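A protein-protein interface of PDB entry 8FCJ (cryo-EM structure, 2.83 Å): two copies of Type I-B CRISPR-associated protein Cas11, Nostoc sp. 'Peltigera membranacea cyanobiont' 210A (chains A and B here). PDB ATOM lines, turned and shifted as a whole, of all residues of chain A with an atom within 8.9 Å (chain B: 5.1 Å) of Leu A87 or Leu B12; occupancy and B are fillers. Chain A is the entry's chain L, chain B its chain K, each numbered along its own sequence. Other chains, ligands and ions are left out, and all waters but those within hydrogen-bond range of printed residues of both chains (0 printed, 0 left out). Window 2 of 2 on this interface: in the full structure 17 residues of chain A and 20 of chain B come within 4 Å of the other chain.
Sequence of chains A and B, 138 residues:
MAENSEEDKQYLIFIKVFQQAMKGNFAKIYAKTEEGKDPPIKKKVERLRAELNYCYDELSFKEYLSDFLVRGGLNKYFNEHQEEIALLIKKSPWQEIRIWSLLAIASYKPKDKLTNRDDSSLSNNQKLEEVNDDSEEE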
ATOM      1  N   GLU A   7      -0.549 -11.605   3.432  1.00  0.00           N
ATOM      2  CA  GLU A   7      -1.858 -11.626   2.789  1.00  0.00           C
ATOM      3  C   GLU A   7      -1.726 -11.866   1.293  1.00  0.00           C
ATOM      4  O   GLU A   7      -2.490 -12.643   0.710  1.00  0.00           O
ATOM      5  CB  GLU A   7      -2.597 -10.314   3.056  1.00  0.00           C
ATOM      6  CG  GLU A   7      -2.704  -9.941   4.524  1.00  0.00           C
ATOM      7  CD  GLU A   7      -3.486 -10.954   5.338  1.00  0.00           C
ATOM      8  OE1 GLU A   7      -4.348 -11.651   4.760  1.00  0.00           O
ATOM      9  OE2 GLU A   7      -3.237 -11.055   6.556  1.00  0.00           O
ATOM     10  N   GLN A  10      -0.879 -15.584   0.731  1.00  0.00           N
ATOM     11  CA  GLN A  10      -2.052 -16.446   0.831  1.00  0.00           C
ATOM     12  C   GLN A  10      -2.984 -16.248  -0.357  1.00  0.00           C
ATOM     13  O   GLN A  10      -3.594 -17.207  -0.840  1.00  0.00           O
ATOM     14  CB  GLN A  10      -2.795 -16.197   2.142  1.00  0.00           C
ATOM     15  CG  GLN A  10      -1.913 -16.205   3.372  1.00  0.00           C
ATOM     16  CD  GLN A  10      -2.658 -15.784   4.618  1.00  0.00           C
ATOM     17  OE1 GLN A  10      -3.816 -15.372   4.553  1.00  0.00           O
ATOM     18  NE2 GLN A  10      -1.998 -15.884   5.765  1.00  0.00           N
ATOM     19  N   LYS A  62     -19.715 -20.485  -0.629  1.00  0.00           N
ATOM     20  CA  LYS A  62     -18.677 -21.280   0.012  1.00  0.00           C
ATOM     21  C   LYS A  62     -18.934 -22.771  -0.152  1.00  0.00           C
ATOM     22  O   LYS A  62     -17.984 -23.545  -0.307  1.00  0.00           O
ATOM     23  CB  LYS A  62     -18.556 -20.898   1.484  1.00  0.00           C
ATOM     24  CG  LYS A  62     -17.674 -19.682   1.695  1.00  0.00           C
ATOM     25  CD  LYS A  62     -17.689 -19.201   3.128  1.00  0.00           C
ATOM     26  CE  LYS A  62     -16.918 -17.901   3.259  1.00  0.00           C
ATOM     27  NZ  LYS A  62     -16.938 -17.376   4.648  1.00  0.00           N
ATOM     28  N   PHE A  78      -2.946 -26.781  -1.774  1.00  0.00           N
ATOM     29  CA  PHE A  78      -3.732 -26.914  -0.552  1.00  0.00           C
ATOM     30  C   PHE A  78      -3.107 -27.905   0.422  1.00  0.00           C
ATOM     31  O   PHE A  78      -3.182 -27.700   1.639  1.00  0.00           O
ATOM     32  CB  PHE A  78      -5.162 -27.336  -0.889  1.00  0.00           C
ATOM     33  CG  PHE A  78      -6.199 -26.765   0.034  1.00  0.00           C
ATOM     34  CD1 PHE A  78      -5.832 -26.145   1.214  1.00  0.00           C
ATOM     35  CD2 PHE A  78      -7.544 -26.854  -0.275  1.00  0.00           C
ATOM     36  CE1 PHE A  78      -6.783 -25.626   2.065  1.00  0.00           C
ATOM     37  CE2 PHE A  78      -8.500 -26.334   0.573  1.00  0.00           C
ATOM     38  CZ  PHE A  78      -8.117 -25.719   1.744  1.00  0.00           C
ATOM     39  N   HIS A  81      -0.591 -25.950   2.426  1.00  0.00           N
ATOM     40  CA  HIS A  81      -1.055 -24.772   3.159  1.00  0.00           C
ATOM     41  C   HIS A  81      -2.440 -24.996   3.761  1.00  0.00           C
ATOM     42  O   HIS A  81      -3.368 -24.221   3.526  1.00  0.00           O
ATOM     43  CB  HIS A  81      -1.060 -23.538   2.260  1.00  0.00           C
ATOM     44  CG  HIS A  81       0.247 -23.274   1.583  1.00  0.00           C
ATOM     45  ND1 HIS A  81       0.613 -23.885   0.405  1.00  0.00           N
ATOM     46  CD2 HIS A  81       1.274 -22.456   1.917  1.00  0.00           C
ATOM     47  CE1 HIS A  81       1.810 -23.459   0.042  1.00  0.00           C
ATOM     48  NE2 HIS A  81       2.233 -22.591   0.944  1.00  0.00           N
ATOM     49  N   GLN A  82      -2.609 -26.084   4.520  1.00  0.00           N
ATOM     50  CA  GLN A  82      -3.893 -26.372   5.157  1.00  0.00           C
ATOM     51  C   GLN A  82      -4.462 -25.170   5.899  1.00  0.00           C
ATOM     52  O   GLN A  82      -5.511 -24.633   5.527  1.00  0.00           O
ATOM     53  CB  GLN A  82      -3.774 -27.503   6.182  1.00  0.00           C
ATOM     54  CG  GLN A  82      -3.796 -28.917   5.667  1.00  0.00           C
ATOM     55  CD  GLN A  82      -2.408 -29.488   5.528  1.00  0.00           C
ATOM     56  OE1 GLN A  82      -1.439 -28.758   5.321  1.00  0.00           O
ATOM     57  NE2 GLN A  82      -2.292 -30.791   5.722  1.00  0.00           N
ATOM     58  N   GLU A  83      -3.757 -24.743   6.948  1.00  0.00           N
ATOM     59  CA  GLU A  83      -4.325 -23.788   7.893  1.00  0.00           C
ATOM     60  C   GLU A  83      -4.523 -22.421   7.258  1.00  0.00           C
ATOM     61  O   GLU A  83      -5.575 -21.799   7.438  1.00  0.00           O
ATOM     62  CB  GLU A  83      -3.435 -23.687   9.133  1.00  0.00           C
ATOM     63  CG  GLU A  83      -1.953 -23.499   8.838  1.00  0.00           C
ATOM     64  CD  GLU A  83      -1.220 -24.811   8.628  1.00  0.00           C
ATOM     65  OE1 GLU A  83      -1.892 -25.846   8.439  1.00  0.00           O
ATOM     66  OE2 GLU A  83       0.029 -24.806   8.649  1.00  0.00           O
ATOM     67  N   GLU A  84      -3.533 -21.942   6.504  1.00  0.00           N
ATOM     68  CA  GLU A  84      -3.621 -20.602   5.932  1.00  0.00           C
ATOM     69  C   GLU A  84      -4.793 -20.491   4.968  1.00  0.00           C
ATOM     70  O   GLU A  84      -5.629 -19.590   5.092  1.00  0.00           O
ATOM     71  CB  GLU A  84      -2.309 -20.249   5.233  1.00  0.00           C
ATOM     72  CG  GLU A  84      -1.116 -20.180   6.167  1.00  0.00           C
ATOM     73  CD  GLU A  84      -0.346 -21.481   6.220  1.00  0.00           C
ATOM     74  OE1 GLU A  84      -0.644 -22.382   5.411  1.00  0.00           O
ATOM     75  OE2 GLU A  84       0.556 -21.604   7.074  1.00  0.00           O
ATOM     76  N   ILE A  85      -4.881 -21.412   4.008  1.00  0.00           N
ATOM     77  CA  ILE A  85      -5.940 -21.340   3.008  1.00  0.00           C
ATOM     78  C   ILE A  85      -7.298 -21.630   3.635  1.00  0.00           C
ATOM     79  O   ILE A  85      -8.306 -21.015   3.271  1.00  0.00           O
ATOM     80  CB  ILE A  85      -5.632 -22.288   1.838  1.00  0.00           C
ATOM     81  CG1 ILE A  85      -4.342 -21.859   1.146  1.00  0.00           C
ATOM     82  CG2 ILE A  85      -6.769 -22.286   0.836  1.00  0.00           C
ATOM     83  CD1 ILE A  85      -4.365 -20.427   0.672  1.00  0.00           C
ATOM     84  N   ALA A  86      -7.351 -22.567   4.585  1.00  0.00           N
ATOM     85  CA  ALA A  86      -8.617 -22.866   5.245  1.00  0.00           C
ATOM     86  C   ALA A  86      -9.140 -21.651   6.001  1.00  0.00           C
ATOM     87  O   ALA A  86     -10.324 -21.305   5.906  1.00  0.00           O
ATOM     88  CB  ALA A  86      -8.446 -24.059   6.184  1.00  0.00           C
ATOM     89  N   LEU A  87      -8.260 -20.975   6.745  1.00  0.00           N
ATOM     90  CA  LEU A  87      -8.666 -19.772   7.459  1.00  0.00           C
ATOM     91  C   LEU A  87      -9.040 -18.658   6.493  1.00  0.00           C
ATOM     92  O   LEU A  87      -9.972 -17.891   6.754  1.00  0.00           O
ATOM     93  CB  LEU A  87      -7.546 -19.317   8.391  1.00  0.00           C
ATOM     94  CG  LEU A  87      -7.430 -20.076   9.710  1.00  0.00           C
ATOM     95  CD1 LEU A  87      -6.016 -19.988  10.250  1.00  0.00           C
ATOM     96  CD2 LEU A  87      -8.426 -19.537  10.714  1.00  0.00           C
ATOM     97  N   LEU A  88      -8.317 -18.546   5.376  1.00  0.00           N
ATOM     98  CA  LEU A  88      -8.636 -17.521   4.389  1.00  0.00           C
ATOM     99  C   LEU A  88     -10.026 -17.735   3.805  1.00  0.00           C
ATOM    100  O   LEU A  88     -10.790 -16.779   3.636  1.00  0.00           O
ATOM    101  CB  LEU A  88      -7.582 -17.522   3.283  1.00  0.00           C
ATOM    102  CG  LEU A  88      -7.752 -16.488   2.174  1.00  0.00           C
ATOM    103  CD1 LEU A  88      -7.120 -15.173   2.585  1.00  0.00           C
ATOM    104  CD2 LEU A  88      -7.144 -16.996   0.882  1.00  0.00           C
ATOM    105  N   ILE A  89     -10.369 -18.984   3.491  1.00  0.00           N
ATOM    106  CA  ILE A  89     -11.695 -19.272   2.956  1.00  0.00           C
ATOM    107  C   ILE A  89     -12.763 -19.028   4.014  1.00  0.00           C
ATOM    108  O   ILE A  89     -13.816 -18.446   3.727  1.00  0.00           O
ATOM    109  CB  ILE A  89     -11.752 -20.709   2.408  1.00  0.00           C
ATOM    110  CG1 ILE A  89     -11.164 -20.761   1.000  1.00  0.00           C
ATOM    111  CG2 ILE A  89     -13.180 -21.218   2.385  1.00  0.00           C
ATOM    112  CD1 ILE A  89     -10.451 -22.050   0.690  1.00  0.00           C
ATOM    113  N   LYS A  90     -12.514 -19.459   5.253  1.00  0.00           N
ATOM    114  CA  LYS A  90     -13.526 -19.321   6.296  1.00  0.00           C
ATOM    115  C   LYS A  90     -13.776 -17.859   6.655  1.00  0.00           C
ATOM    116  O   LYS A  90     -14.921 -17.466   6.905  1.00  0.00           O
ATOM    117  CB  LYS A  90     -13.109 -20.108   7.536  1.00  0.00           C
ATOM    118  CG  LYS A  90     -14.227 -20.315   8.540  1.00  0.00           C
ATOM    119  CD  LYS A  90     -13.765 -20.012   9.953  1.00  0.00           C
ATOM    120  CE  LYS A  90     -14.754 -20.536  10.977  1.00  0.00           C
ATOM    121  NZ  LYS A  90     -16.157 -20.228  10.591  1.00  0.00           N
ATOM    122  N   LYS A  91     -12.725 -17.043   6.685  1.00  0.00           N
ATOM    123  CA  LYS A  91     -12.809 -15.686   7.213  1.00  0.00           C
ATOM    124  C   LYS A  91     -13.243 -14.662   6.169  1.00  0.00           C
ATOM    125  O   LYS A  91     -14.119 -13.834   6.437  1.00  0.00           O
ATOM    126  CB  LYS A  91     -11.458 -15.272   7.795  1.00  0.00           C
ATOM    127  CG  LYS A  91     -11.181 -15.780   9.193  1.00  0.00           C
ATOM    128  CD  LYS A  91      -9.813 -15.314   9.653  1.00  0.00           C
ATOM    129  CE  LYS A  91      -9.650 -15.460  11.150  1.00  0.00           C
ATOM    130  NZ  LYS A  91      -8.260 -15.148  11.582  1.00  0.00           N
ATOM    131  N   SER A  92     -12.636 -14.698   4.986  1.00  0.00           N
ATOM    132  CA  SER A  92     -12.788 -13.615   4.029  1.00  0.00           C
ATOM    133  C   SER A  92     -14.233 -13.507   3.544  1.00  0.00           C
ATOM    134  O   SER A  92     -14.958 -14.504   3.497  1.00  0.00           O
ATOM    135  CB  SER A  92     -11.861 -13.828   2.837  1.00  0.00           C
ATOM    136  OG  SER A  92     -10.508 -13.875   3.251  1.00  0.00           O
ATOM    137  N   PRO A  93     -14.681 -12.299   3.204  1.00  0.00           N
ATOM    138  CA  PRO A  93     -16.019 -12.147   2.622  1.00  0.00           C
ATOM    139  C   PRO A  93     -16.129 -12.914   1.314  1.00  0.00           C
ATOM    140  O   PRO A  93     -15.178 -12.988   0.535  1.00  0.00           O
ATOM    141  CB  PRO A  93     -16.145 -10.636   2.403  1.00  0.00           C
ATOM    142  CG  PRO A  93     -15.138 -10.029   3.317  1.00  0.00           C
ATOM    143  CD  PRO A  93     -14.007 -11.003   3.384  1.00  0.00           C
ATOM    144  N   ILE A  97     -13.638 -13.599  -2.227  1.00  0.00           N
ATOM    145  CA  ILE A  97     -13.205 -14.923  -2.656  1.00  0.00           C
ATOM    146  C   ILE A  97     -13.696 -15.209  -4.068  1.00  0.00           C
ATOM    147  O   ILE A  97     -12.988 -15.826  -4.871  1.00  0.00           O
ATOM    148  CB  ILE A  97     -13.675 -15.996  -1.659  1.00  0.00           C
ATOM    149  CG1 ILE A  97     -13.092 -15.730  -0.275  1.00  0.00           C
ATOM    150  CG2 ILE A  97     -13.250 -17.372  -2.122  1.00  0.00           C
ATOM    151  CD1 ILE A  97     -14.025 -16.093   0.848  1.00  0.00           C
ATOM    152  N   TRP A 100     -11.376 -13.380  -6.406  1.00  0.00           N
ATOM    153  CA  TRP A 100     -10.120 -14.109  -6.569  1.00  0.00           C
ATOM    154  C   TRP A 100     -10.308 -15.344  -7.441  1.00  0.00           C
ATOM    155  O   TRP A 100      -9.446 -15.668  -8.266  1.00  0.00           O
ATOM    156  CB  TRP A 100      -9.550 -14.503  -5.209  1.00  0.00           C
ATOM    157  CG  TRP A 100      -9.427 -13.373  -4.245  1.00  0.00           C
ATOM    158  CD1 TRP A 100      -9.387 -12.044  -4.540  1.00  0.00           C
ATOM    159  CD2 TRP A 100      -9.321 -13.474  -2.823  1.00  0.00           C
ATOM    160  NE1 TRP A 100      -9.268 -11.308  -3.388  1.00  0.00           N
ATOM    161  CE2 TRP A 100      -9.224 -12.164  -2.319  1.00  0.00           C
ATOM    162  CE3 TRP A 100      -9.301 -14.544  -1.927  1.00  0.00           C
ATOM    163  CZ2 TRP A 100      -9.109 -11.897  -0.959  1.00  0.00           C
ATOM    164  CZ3 TRP A 100      -9.187 -14.277  -0.580  1.00  0.00           C
ATOM    165  CH2 TRP A 100      -9.092 -12.964  -0.109  1.00  0.00           C
ATOM    166  N   GLU B   7     -12.823 -19.707  17.972  1.00  0.00           N
ATOM    167  CA  GLU B   7     -13.580 -20.323  16.886  1.00  0.00           C
ATOM    168  C   GLU B   7     -12.657 -20.830  15.787  1.00  0.00           C
ATOM    169  O   GLU B   7     -12.861 -21.925  15.251  1.00  0.00           O
ATOM    170  CB  GLU B   7     -14.592 -19.328  16.318  1.00  0.00           C
ATOM    171  CG  GLU B   7     -15.621 -18.839  17.322  1.00  0.00           C
ATOM    172  CD  GLU B   7     -15.124 -17.666  18.143  1.00  0.00           C
ATOM    173  OE1 GLU B   7     -14.149 -17.012  17.717  1.00  0.00           O
ATOM    174  OE2 GLU B   7     -15.706 -17.399  19.216  1.00  0.00           O
ATOM    175  N   ASP B   8     -11.634 -20.049  15.439  1.00  0.00           N
ATOM    176  CA  ASP B   8     -10.700 -20.472  14.403  1.00  0.00           C
ATOM    177  C   ASP B   8      -9.910 -21.703  14.833  1.00  0.00           C
ATOM    178  O   ASP B   8      -9.690 -22.615  14.028  1.00  0.00           O
ATOM    179  CB  ASP B   8      -9.758 -19.325  14.052  1.00  0.00           C
ATOM    180  CG  ASP B   8     -10.498 -18.042  13.745  1.00  0.00           C
ATOM    181  OD1 ASP B   8     -11.683 -18.116  13.360  1.00  0.00           O
ATOM    182  OD2 ASP B   8      -9.898 -16.959  13.899  1.00  0.00           O
ATOM    183  N   LYS B   9      -9.466 -21.744  16.091  1.00  0.00           N
ATOM    184  CA  LYS B   9      -8.750 -22.918  16.578  1.00  0.00           C
ATOM    185  C   LYS B   9      -9.640 -24.151  16.553  1.00  0.00           C
ATOM    186  O   LYS B   9      -9.202 -25.235  16.147  1.00  0.00           O
ATOM    187  CB  LYS B   9      -8.221 -22.670  17.989  1.00  0.00           C
ATOM    188  CG  LYS B   9      -7.287 -21.483  18.109  1.00  0.00           C
ATOM    189  CD  LYS B   9      -7.198 -21.002  19.548  1.00  0.00           C
ATOM    190  CE  LYS B   9      -6.365 -19.738  19.658  1.00  0.00           C
ATOM    191  NZ  LYS B   9      -6.367 -19.191  21.043  1.00  0.00           N
ATOM    192  N   GLN B  10     -10.895 -24.005  16.986  1.00  0.00           N
ATOM    193  CA  GLN B  10     -11.818 -25.133  16.955  1.00  0.00           C
ATOM    194  C   GLN B  10     -12.054 -25.606  15.529  1.00  0.00           C
ATOM    195  O   GLN B  10     -12.090 -26.812  15.267  1.00  0.00           O
ATOM    196  CB  GLN B  10     -13.140 -24.756  17.619  1.00  0.00           C
ATOM    197  CG  GLN B  10     -13.047 -24.553  19.117  1.00  0.00           C
ATOM    198  CD  GLN B  10     -14.332 -24.015  19.710  1.00  0.00           C
ATOM    199  OE1 GLN B  10     -15.307 -23.784  18.997  1.00  0.00           O
ATOM    200  NE2 GLN B  10     -14.340 -23.814  21.021  1.00  0.00           N
ATOM    201  N   TYR B  11     -12.205 -24.670  14.592  1.00  0.00           N
ATOM    202  CA  TYR B  11     -12.411 -25.035  13.195  1.00  0.00           C
ATOM    203  C   TYR B  11     -11.200 -25.772  12.630  1.00  0.00           C
ATOM    204  O   TYR B  11     -11.345 -26.791  11.942  1.00  0.00           O
ATOM    205  CB  TYR B  11     -12.728 -23.772  12.393  1.00  0.00           C
ATOM    206  CG  TYR B  11     -12.423 -23.827  10.916  1.00  0.00           C
ATOM    207  CD1 TYR B  11     -13.257 -24.505  10.041  1.00  0.00           C
ATOM    208  CD2 TYR B  11     -11.321 -23.169  10.393  1.00  0.00           C
ATOM    209  CE1 TYR B  11     -12.989 -24.544   8.690  1.00  0.00           C
ATOM    210  CE2 TYR B  11     -11.045 -23.203   9.045  1.00  0.00           C
ATOM    211  CZ  TYR B  11     -11.882 -23.891   8.198  1.00  0.00           C
ATOM    212  OH  TYR B  11     -11.610 -23.927   6.853  1.00  0.00           O
ATOM    213  N   LEU B  12      -9.994 -25.290  12.937  1.00  0.00           N
ATOM    214  CA  LEU B  12      -8.786 -25.937  12.433  1.00  0.00           C
ATOM    215  C   LEU B  12      -8.629 -27.342  12.999  1.00  0.00           C
ATOM    216  O   LEU B  12      -8.319 -28.294  12.269  1.00  0.00           O
ATOM    217  CB  LEU B  12      -7.562 -25.085  12.764  1.00  0.00           C
ATOM    218  CG  LEU B  12      -7.397 -23.802  11.951  1.00  0.00           C
ATOM    219  CD1 LEU B  12      -6.060 -23.154  12.251  1.00  0.00           C
ATOM    220  CD2 LEU B  12      -7.532 -24.095  10.469  1.00  0.00           C
ATOM    221  N   ILE B  13      -8.848 -27.504  14.305  1.00  0.00           N
ATOM    222  CA  ILE B  13      -8.653 -28.834  14.869  1.00  0.00           C
ATOM    223  C   ILE B  13      -9.817 -29.761  14.529  1.00  0.00           C
ATOM    224  O   ILE B  13      -9.638 -30.982  14.519  1.00  0.00           O
ATOM    225  CB  ILE B  13      -8.313 -28.720  16.373  1.00  0.00           C
ATOM    226  CG1 ILE B  13      -9.444 -28.161  17.246  1.00  0.00           C
ATOM    227  CG2 ILE B  13      -7.056 -27.882  16.567  1.00  0.00           C
ATOM    228  CD1 ILE B  13     -10.626 -29.040  17.441  1.00  0.00           C
ATOM    229  N   PHE B  14     -10.991 -29.223  14.184  1.00  0.00           N
ATOM    230  CA  PHE B  14     -12.035 -30.066  13.608  1.00  0.00           C
ATOM    231  C   PHE B  14     -11.649 -30.536  12.214  1.00  0.00           C
ATOM    232  O   PHE B  14     -11.955 -31.671  11.828  1.00  0.00           O
ATOM    233  CB  PHE B  14     -13.365 -29.317  13.561  1.00  0.00           C
ATOM    234  CG  PHE B  14     -14.385 -29.963  12.667  1.00  0.00           C
ATOM    235  CD1 PHE B  14     -15.111 -31.055  13.104  1.00  0.00           C
ATOM    236  CD2 PHE B  14     -14.611 -29.486  11.390  1.00  0.00           C
ATOM    237  CE1 PHE B  14     -16.044 -31.656  12.284  1.00  0.00           C
ATOM    238  CE2 PHE B  14     -15.543 -30.085  10.567  1.00  0.00           C
ATOM    239  CZ  PHE B  14     -16.259 -31.170  11.016  1.00  0.00           C
ATOM    240  N   ILE B  15     -10.998 -29.670  11.436  1.00  0.00           N
ATOM    241  CA  ILE B  15     -10.456 -30.100  10.150  1.00  0.00           C
ATOM    242  C   ILE B  15      -9.460 -31.233  10.357  1.00  0.00           C
ATOM    243  O   ILE B  15      -9.454 -32.223   9.617  1.00  0.00           O
ATOM    244  CB  ILE B  15      -9.819 -28.909   9.413  1.00  0.00           C
ATOM    245  CG1 ILE B  15     -10.900 -28.043   8.767  1.00  0.00           C
ATOM    246  CG2 ILE B  15      -8.826 -29.390   8.370  1.00  0.00           C
ATOM    247  CD1 ILE B  15     -10.355 -27.005   7.817  1.00  0.00           C
ATOM    248  N   LYS B  16      -8.607 -31.105  11.376  1.00  0.00           N
ATOM    249  CA  LYS B  16      -7.667 -32.178  11.692  1.00  0.00           C
ATOM    250  C   LYS B  16      -8.396 -33.459  12.087  1.00  0.00           C
ATOM    251  O   LYS B  16      -7.994 -34.561  11.691  1.00  0.00           O
ATOM    252  CB  LYS B  16      -6.720 -31.738  12.807  1.00  0.00           C
ATOM    253  CG  LYS B  16      -5.668 -30.738  12.368  1.00  0.00           C
ATOM    254  CD  LYS B  16      -4.986 -30.103  13.565  1.00  0.00           C
ATOM    255  CE  LYS B  16      -4.281 -28.815  13.178  1.00  0.00           C
ATOM    256  NZ  LYS B  16      -3.900 -28.015  14.374  1.00  0.00           N
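The backbone carbonyl oxygen of Ala A86 sits at hydrogen-bond distance from the side-chain hydroxyl of Tyr B11. The side-chain amino group (NZ) of Lys A91 lies within salt-bridge range of the side-chain carboxylate (OD2) of Asp B8, at 3.4 Å.
Ala A86 touches Ile B15. Leu A87 touches Asp B8 (CD2 to CB, 3.6 Å). Leu B12 touches Leu A87.
Of the printed residues of chain B, Ala A86 touches Tyr B11 and Ile B15. Leu A87 touches just these residues of chain B: Asp B8 (3.6 Å) and Leu B12 (3.7 Å). Of the printed residues of chain B, Lys A91 touches Asp B8. Printed residues of chain A within 4 Å of Asp B8: Leu A87 and Lys A91. Of the printed residues of chain A, Tyr B11 touches Ala A86 (3.1 Å). Of the printed residues of chain A, Leu B12 touches Leu A87. Ile B13 touches none of the printed residues of chain A. Of the printed residues of chain A, Ile B15 touches Ala A86 (3.9 Å). The nearest residue of chain B that does not touch Leu A87 is Tyr B11 (4.2 Å).
Of the 10 printed residues of chain B, 4 touch a printed residue of chain A. Hydrophobic or aromatic side chains of chain A that line the printed part of chain B: Ala A86 and Leu A87. Along chain A the printed residues that touch a printed residue of chain B span positions 86 to 91. Among the printed residues, 5 pairs touch across the chains. Among the printed residues, Asp or Glu carboxylates within 4 Å of a Lys or Arg side-chain nitrogen of the other chain: Lys A91 with Asp B8 (3.4 Å).
2 positions are printed for both chains. Of the 5 pairs that touch across the chains among the printed residues, none has its exchanged pair printed and touching as well.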
